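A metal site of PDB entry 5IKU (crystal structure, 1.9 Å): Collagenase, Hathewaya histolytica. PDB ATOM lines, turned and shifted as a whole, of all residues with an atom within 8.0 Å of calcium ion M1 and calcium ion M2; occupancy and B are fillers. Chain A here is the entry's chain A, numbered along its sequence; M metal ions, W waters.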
ATOM      1  N   GLU A  12     -26.338 -23.323 -26.946  1.00  0.00           N
ATOM      2  CA  GLU A  12     -25.131 -22.582 -26.570  1.00  0.00           C
ATOM      3  C   GLU A  12     -24.611 -23.073 -25.223  1.00  0.00           C
ATOM      4  O   GLU A  12     -25.342 -23.698 -24.453  1.00  0.00           O
ATOM      5  CB  GLU A  12     -25.413 -21.065 -26.533  1.00  0.00           C
ATOM      6  CG  GLU A  12     -26.397 -20.683 -25.466  1.00  0.00           C
ATOM      7  CD  GLU A  12     -26.388 -19.198 -25.226  1.00  0.00           C
ATOM      8  OE1 GLU A  12     -25.320 -18.553 -25.385  1.00  0.00           O
ATOM      9  OE2 GLU A  12     -27.452 -18.686 -24.817  1.00  0.00           O
ATOM     10  N   MET A  13     -23.352 -22.779 -24.923  1.00  0.00           N
ATOM     11  CA  MET A  13     -22.768 -23.121 -23.636  1.00  0.00           C
ATOM     12  C   MET A  13     -21.910 -21.926 -23.194  1.00  0.00           C
ATOM     13  O   MET A  13     -20.875 -21.646 -23.780  1.00  0.00           O
ATOM     14  CB  MET A  13     -21.986 -24.449 -23.834  1.00  0.00           C
ATOM     15  CG  MET A  13     -21.038 -24.913 -22.742  1.00  0.00           C
ATOM     16  SD  MET A  13     -20.642 -26.647 -23.044  1.00  0.00           S
ATOM     17  CE  MET A  13     -22.293 -27.381 -23.070  1.00  0.00           C
ATOM     18  N   GLU A  14     -22.340 -21.189 -22.172  1.00  0.00           N
ATOM     19  CA  GLU A  14     -21.603 -20.018 -21.705  1.00  0.00           C
ATOM     20  C   GLU A  14     -20.326 -20.454 -20.961  1.00  0.00           C
ATOM     21  O   GLU A  14     -20.315 -21.536 -20.392  1.00  0.00           O
ATOM     22  CB  GLU A  14     -22.523 -19.183 -20.773  1.00  0.00           C
ATOM     23  CG  GLU A  14     -23.725 -18.604 -21.543  1.00  0.00           C
ATOM     24  CD  GLU A  14     -23.362 -17.406 -22.410  1.00  0.00           C
ATOM     25  OE1 GLU A  14     -22.205 -16.912 -22.312  1.00  0.00           O
ATOM     26  OE2 GLU A  14     -24.237 -16.921 -23.191  1.00  0.00           O
ATOM     27  N   PRO A  15     -19.257 -19.667 -20.940  1.00  0.00           N
ATOM     28  CA  PRO A  15     -19.164 -18.382 -21.604  1.00  0.00           C
ATOM     29  C   PRO A  15     -18.822 -18.555 -23.077  1.00  0.00           C
ATOM     30  O   PRO A  15     -18.046 -19.427 -23.440  1.00  0.00           O
ATOM     31  CB  PRO A  15     -17.982 -17.700 -20.881  1.00  0.00           C
ATOM     32  CG  PRO A  15     -17.103 -18.850 -20.519  1.00  0.00           C
ATOM     33  CD  PRO A  15     -18.029 -19.993 -20.183  1.00  0.00           C
ATOM     34  N   ASN A  16     -19.423 -17.742 -23.933  1.00  0.00           N
ATOM     35  CA  ASN A  16     -19.087 -17.831 -25.374  1.00  0.00           C
ATOM     36  C   ASN A  16     -19.014 -16.389 -25.947  1.00  0.00           C
ATOM     37  O   ASN A  16     -19.448 -16.126 -27.038  1.00  0.00           O
ATOM     38  CB  ASN A  16     -20.179 -18.634 -26.075  1.00  0.00           C
ATOM     39  CG  ASN A  16     -21.524 -18.078 -25.810  1.00  0.00           C
ATOM     40  OD1 ASN A  16     -21.620 -16.970 -25.290  1.00  0.00           O
ATOM     41  ND2 ASN A  16     -22.592 -18.839 -26.120  1.00  0.00           N
ATOM     42  N   ASP A  17     -18.425 -15.453 -25.178  1.00  0.00           N
ATOM     43  CA  ASP A  17     -18.642 -14.016 -25.381  1.00  0.00           C
ATOM     44  C   ASP A  17     -17.753 -13.307 -26.438  1.00  0.00           C
ATOM     45  O   ASP A  17     -17.950 -12.136 -26.754  1.00  0.00           O
ATOM     46  CB  ASP A  17     -18.611 -13.268 -24.051  1.00  0.00           C
ATOM     47  CG  ASP A  17     -19.782 -13.628 -23.139  1.00  0.00           C
ATOM     48  OD1 ASP A  17     -19.706 -13.145 -21.998  1.00  0.00           O
ATOM     49  OD2 ASP A  17     -20.753 -14.351 -23.533  1.00  0.00           O
ATOM     50  N   ASP A  18     -16.774 -14.036 -26.973  1.00  0.00           N
ATOM     51  CA  ASP A  18     -15.912 -13.523 -28.028  1.00  0.00           C
ATOM     52  C   ASP A  18     -15.402 -14.670 -28.863  1.00  0.00           C
ATOM     53  O   ASP A  18     -15.711 -15.847 -28.575  1.00  0.00           O
ATOM     54  CB  ASP A  18     -14.746 -12.669 -27.468  1.00  0.00           C
ATOM     55  CG  ASP A  18     -13.719 -13.493 -26.691  1.00  0.00           C
ATOM     56  OD1 ASP A  18     -12.848 -12.888 -26.043  1.00  0.00           O
ATOM     57  OD2 ASP A  18     -13.764 -14.736 -26.712  1.00  0.00           O
ATOM     58  N   GLU A  21     -13.668 -17.860 -27.417  1.00  0.00           N
ATOM     59  CA  GLU A  21     -14.468 -18.893 -26.732  1.00  0.00           C
ATOM     60  C   GLU A  21     -15.772 -19.202 -27.486  1.00  0.00           C
ATOM     61  O   GLU A  21     -16.750 -19.623 -26.870  1.00  0.00           O
ATOM     62  CB  GLU A  21     -14.722 -18.544 -25.257  1.00  0.00           C
ATOM     63  CG  GLU A  21     -14.938 -17.065 -25.025  1.00  0.00           C
ATOM     64  CD  GLU A  21     -14.979 -16.669 -23.545  1.00  0.00           C
ATOM     65  OE1 GLU A  21     -14.116 -17.138 -22.770  1.00  0.00           O
ATOM     66  OE2 GLU A  21     -15.900 -15.866 -23.202  1.00  0.00           O
ATOM     67  N   ASN A  23     -18.805 -20.991 -29.283  1.00  0.00           N
ATOM     68  CA  ASN A  23     -19.310 -22.386 -29.266  1.00  0.00           C
ATOM     69  C   ASN A  23     -19.371 -22.920 -30.720  1.00  0.00           C
ATOM     70  O   ASN A  23     -19.673 -22.180 -31.648  1.00  0.00           O
ATOM     71  CB  ASN A  23     -20.706 -22.464 -28.688  1.00  0.00           C
ATOM     72  CG  ASN A  23     -20.816 -21.952 -27.250  1.00  0.00           C
ATOM     73  OD1 ASN A  23     -21.839 -21.393 -26.893  1.00  0.00           O
ATOM     74  ND2 ASN A  23     -19.794 -22.177 -26.416  1.00  0.00           N
ATOM     75  N   LYS A  33     -30.177 -23.177 -30.142  1.00  0.00           N
ATOM     76  CA  LYS A  33     -30.947 -22.232 -29.335  1.00  0.00           C
ATOM     77  C   LYS A  33     -30.028 -21.524 -28.385  1.00  0.00           C
ATOM     78  O   LYS A  33     -29.045 -22.097 -27.919  1.00  0.00           O
ATOM     79  CB  LYS A  33     -32.012 -22.923 -28.492  1.00  0.00           C
ATOM     80  CG  LYS A  33     -33.142 -23.543 -29.284  1.00  0.00           C
ATOM     81  CD  LYS A  33     -34.308 -23.911 -28.368  1.00  0.00           C
ATOM     82  CE  LYS A  33     -35.401 -24.598 -29.168  1.00  0.00           C
ATOM     83  NZ  LYS A  33     -35.562 -23.940 -30.499  1.00  0.00           N
ATOM     84  N   GLY A  34     -30.345 -20.271 -28.094  1.00  0.00           N
ATOM     85  CA  GLY A  34     -29.686 -19.569 -27.012  1.00  0.00           C
ATOM     86  C   GLY A  34     -30.465 -18.327 -26.599  1.00  0.00           C
ATOM     87  O   GLY A  34     -31.559 -18.076 -27.075  1.00  0.00           O
ATOM     88  N   ASP A  35     -29.899 -17.519 -25.714  1.00  0.00           N
ATOM     89  CA  ASP A  35     -30.589 -16.278 -25.369  1.00  0.00           C
ATOM     90  C   ASP A  35     -29.562 -15.274 -24.904  1.00  0.00           C
ATOM     91  O   ASP A  35     -28.456 -15.655 -24.528  1.00  0.00           O
ATOM     92  CB  ASP A  35     -31.643 -16.497 -24.291  1.00  0.00           C
ATOM     93  CG  ASP A  35     -31.124 -17.339 -23.140  1.00  0.00           C
ATOM     94  OD1 ASP A  35     -30.154 -16.910 -22.471  1.00  0.00           O
ATOM     95  OD2 ASP A  35     -31.673 -18.429 -22.929  1.00  0.00           O
ATOM     96  N   LEU A  36     -29.935 -14.000 -24.940  1.00  0.00           N
ATOM     97  CA  LEU A  36     -29.081 -12.918 -24.454  1.00  0.00           C
ATOM     98  C   LEU A  36     -29.906 -12.194 -23.377  1.00  0.00           C
ATOM     99  O   LEU A  36     -30.436 -11.118 -23.630  1.00  0.00           O
ATOM    100  CB  LEU A  36     -28.792 -11.914 -25.576  1.00  0.00           C
ATOM    101  CG  LEU A  36     -27.966 -12.507 -26.716  1.00  0.00           C
ATOM    102  CD1 LEU A  36     -28.093 -11.528 -27.884  1.00  0.00           C
ATOM    103  CD2 LEU A  36     -26.518 -12.595 -26.255  1.00  0.00           C
ATOM    104  N   ASN A  37     -30.011 -12.803 -22.212  1.00  0.00           N
ATOM    105  CA  ASN A  37     -30.893 -12.283 -21.171  1.00  0.00           C
ATOM    106  C   ASN A  37     -30.038 -11.519 -20.154  1.00  0.00           C
ATOM    107  O   ASN A  37     -28.910 -11.951 -19.856  1.00  0.00           O
ATOM    108  CB  ASN A  37     -31.620 -13.447 -20.461  1.00  0.00           C
ATOM    109  CG  ASN A  37     -32.727 -14.073 -21.315  1.00  0.00           C
ATOM    110  OD1 ASN A  37     -33.313 -13.438 -22.200  1.00  0.00           O
ATOM    111  ND2 ASN A  37     -33.016 -15.326 -21.031  1.00  0.00           N
ATOM    112  N   SER A  39     -27.437  -9.277 -18.342  1.00  0.00           N
ATOM    113  CA  SER A  39     -26.125  -8.743 -18.717  1.00  0.00           C
ATOM    114  C   SER A  39     -25.341  -9.675 -19.658  1.00  0.00           C
ATOM    115  O   SER A  39     -24.190  -9.380 -19.965  1.00  0.00           O
ATOM    116  CB  SER A  39     -25.296  -8.508 -17.461  1.00  0.00           C
ATOM    117  OG  SER A  39     -24.872  -9.768 -16.949  1.00  0.00           O
ATOM    118  N   ASP A  40     -25.923 -10.789 -20.091  1.00  0.00           N
ATOM    119  CA  ASP A  40     -25.235 -11.583 -21.167  1.00  0.00           C
ATOM    120  C   ASP A  40     -25.501 -10.841 -22.484  1.00  0.00           C
ATOM    121  O   ASP A  40     -26.617 -10.908 -23.029  1.00  0.00           O
ATOM    122  CB  ASP A  40     -25.754 -13.018 -21.199  1.00  0.00           C
ATOM    123  CG  ASP A  40     -25.219 -13.803 -22.379  1.00  0.00           C
ATOM    124  OD1 ASP A  40     -24.032 -13.646 -22.720  1.00  0.00           O
ATOM    125  OD2 ASP A  40     -25.991 -14.578 -22.988  1.00  0.00           O
ATOM    126  N   ASP A  41     -24.535 -10.087 -22.992  1.00  0.00           N
ATOM    127  CA  ASP A  41     -24.842  -9.272 -24.164  1.00  0.00           C
ATOM    128  C   ASP A  41     -24.197  -9.691 -25.459  1.00  0.00           C
ATOM    129  O   ASP A  41     -24.391  -9.001 -26.490  1.00  0.00           O
ATOM    130  CB  ASP A  41     -24.627  -7.769 -23.919  1.00  0.00           C
ATOM    131  CG  ASP A  41     -23.208  -7.429 -23.590  1.00  0.00           C
ATOM    132  OD1 ASP A  41     -22.397  -8.372 -23.509  1.00  0.00           O
ATOM    133  OD2 ASP A  41     -22.902  -6.227 -23.405  1.00  0.00           O
ATOM    134  N   ALA A  42     -23.418 -10.787 -25.424  1.00  0.00           N
ATOM    135  CA  ALA A  42     -22.829 -11.292 -26.673  1.00  0.00           C
ATOM    136  C   ALA A  42     -22.662 -12.819 -26.625  1.00  0.00           C
ATOM    137  O   ALA A  42     -22.293 -13.366 -25.604  1.00  0.00           O
ATOM    138  CB  ALA A  42     -21.469 -10.643 -26.891  1.00  0.00           C
ATOM    139  N   ASP A  43     -22.969 -13.468 -27.745  1.00  0.00           N
ATOM    140  CA  ASP A  43     -22.835 -14.920 -27.918  1.00  0.00           C
ATOM    141  C   ASP A  43     -22.109 -15.096 -29.257  1.00  0.00           C
ATOM    142  O   ASP A  43     -22.484 -14.436 -30.236  1.00  0.00           O
ATOM    143  CB  ASP A  43     -24.219 -15.604 -28.039  1.00  0.00           C
ATOM    144  CG  ASP A  43     -24.961 -15.671 -26.712  1.00  0.00           C
ATOM    145  OD1 ASP A  43     -24.321 -15.379 -25.674  1.00  0.00           O
ATOM    146  OD2 ASP A  43     -26.160 -16.040 -26.697  1.00  0.00           O
ATOM    147  N   THR A  44     -21.161 -16.024 -29.295  1.00  0.00           N
ATOM    148  CA  THR A  44     -20.324 -16.266 -30.464  1.00  0.00           C
ATOM    149  C   THR A  44     -20.286 -17.750 -30.792  1.00  0.00           C
ATOM    150  O   THR A  44     -20.151 -18.599 -29.879  1.00  0.00           O
ATOM    151  CB  THR A  44     -18.865 -15.757 -30.235  1.00  0.00           C
ATOM    152  OG1 THR A  44     -18.923 -14.536 -29.504  1.00  0.00           O
ATOM    153  CG2 THR A  44     -18.133 -15.563 -31.579  1.00  0.00           C
ATOM    154  N   PHE A  45     -20.464 -18.057 -32.093  1.00  0.00           N
ATOM    155  CA  PHE A  45     -20.465 -19.416 -32.597  1.00  0.00           C
ATOM    156  C   PHE A  45     -19.556 -19.490 -33.791  1.00  0.00           C
ATOM    157  O   PHE A  45     -19.310 -18.503 -34.453  1.00  0.00           O
ATOM    158  CB  PHE A  45     -21.886 -19.787 -33.085  1.00  0.00           C
ATOM    159  CG  PHE A  45     -22.934 -19.670 -31.997  1.00  0.00           C
ATOM    160  CD1 PHE A  45     -23.646 -18.491 -31.821  1.00  0.00           C
ATOM    161  CD2 PHE A  45     -23.164 -20.746 -31.119  1.00  0.00           C
ATOM    162  CE1 PHE A  45     -24.582 -18.369 -30.794  1.00  0.00           C
ATOM    163  CE2 PHE A  45     -24.100 -20.621 -30.083  1.00  0.00           C
ATOM    164  CZ  PHE A  45     -24.815 -19.428 -29.933  1.00  0.00           C
ATOM    165  N   ILE A 106     -23.337 -12.512 -32.038  1.00  0.00           N
ATOM    166  CA  ILE A 106     -24.655 -11.974 -31.842  1.00  0.00           C
ATOM    167  C   ILE A 106     -24.524 -11.110 -30.594  1.00  0.00           C
ATOM    168  O   ILE A 106     -24.032 -11.592 -29.593  1.00  0.00           O
ATOM    169  CB  ILE A 106     -25.647 -13.105 -31.594  1.00  0.00           C
ATOM    170  CG1 ILE A 106     -25.616 -14.105 -32.721  1.00  0.00           C
ATOM    171  CG2 ILE A 106     -27.073 -12.543 -31.477  1.00  0.00           C
ATOM    172  CD1 ILE A 106     -26.268 -15.418 -32.365  1.00  0.00           C
ATOM    173  N   ILE A 115     -33.685 -11.366 -24.843  1.00  0.00           N
ATOM    174  CA  ILE A 115     -33.846 -11.811 -26.209  1.00  0.00           C
ATOM    175  C   ILE A 115     -33.607 -13.314 -26.196  1.00  0.00           C
ATOM    176  O   ILE A 115     -32.624 -13.768 -25.647  1.00  0.00           O
ATOM    177  CB  ILE A 115     -32.795 -11.133 -27.133  1.00  0.00           C
ATOM    178  CG1 ILE A 115     -32.944  -9.606 -27.073  1.00  0.00           C
ATOM    179  CG2 ILE A 115     -32.877 -11.662 -28.566  1.00  0.00           C
ATOM    180  CD1 ILE A 115     -31.638  -8.919 -27.400  1.00  0.00           C
ATOM    181  N   TYR A 117     -33.388 -16.662 -29.052  1.00  0.00           N
ATOM    182  CA  TYR A 117     -33.264 -16.791 -30.478  1.00  0.00           C
ATOM    183  C   TYR A 117     -33.014 -18.232 -30.812  1.00  0.00           C
ATOM    184  O   TYR A 117     -32.633 -19.056 -29.951  1.00  0.00           O
ATOM    185  CB  TYR A 117     -32.072 -15.963 -31.005  1.00  0.00           C
ATOM    186  CG  TYR A 117     -30.731 -16.324 -30.390  1.00  0.00           C
ATOM    187  CD1 TYR A 117     -29.995 -17.439 -30.861  1.00  0.00           C
ATOM    188  CD2 TYR A 117     -30.212 -15.572 -29.321  1.00  0.00           C
ATOM    189  CE1 TYR A 117     -28.786 -17.784 -30.300  1.00  0.00           C
ATOM    190  CE2 TYR A 117     -28.987 -15.903 -28.755  1.00  0.00           C
ATOM    191  CZ  TYR A 117     -28.285 -17.012 -29.249  1.00  0.00           C
ATOM    192  OH  TYR A 117     -27.083 -17.393 -28.706  1.00  0.00           O
HETATM  193 CA    CA M   1     -26.201 -16.549 -24.307  1.00  0.00          CA
HETATM  194 CA    CA M   2     -22.676 -15.152 -24.035  1.00  0.00          CA
HETATM  195  O   HOH W   1     -27.348 -17.305 -22.168  1.00  0.00           O
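Calcium ion M2 is bound by OD2 of Asp 17 (2.1 Å), OD1 of Asp 43 (2.3 Å), O of Ala 42 (2.4 Å), OD1 of Asp 40 (2.4 Å), OD1 of Asn 16 (2.4 Å), OE2 of Glu 14 (2.5 Å) and OE1 of Glu 14 (2.5 Å).
Calcium ion M1 is bound by the side-chain carboxylate (OE2) of Glu 14, the side-chain carboxylate (OD2) of Asp 40, the backbone carbonyl oxygen (O) of Asp 35, the side-chain carboxylate (OE1) of Glu 12, the side-chain carboxylate (OD2) of Asp 43, the side-chain carboxylate (OE2) of Glu 12, water W1 and the side-chain carboxylate (OD1) of Asp 43.
Of the 24 residues printed, 6 come within 4 Å of calcium ion M2.
N of Asp 17 is in hydrogen-bond range of OE2 of Glu 21 (3.2 Å).
The side-chain carboxylate (OD2) of Asp 43 lies close to the side-chain hydroxyl (OH) of Tyr 117 (2.6 Å).
N of Ile 106 is in hydrogen-bond range of O of Asp 43 (2.8 Å).
The side-chain carboxylate (OE1) of Glu 12 lies close to the side-chain amide nitrogen (ND2) of Asn 16 (2.8 Å).
The backbone NH (N) of Glu 12 is in hydrogen-bond range of the backbone carbonyl oxygen (O) of Lys 33, 3.1 Å away.
N of Thr 44 sits at hydrogen-bond distance from O of Asn 16.
The side-chain amide nitrogen (ND2) of Asn 16 is in hydrogen-bond range of the side-chain amide oxygen (OD1) of Asn 23, 2.8 Å away.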
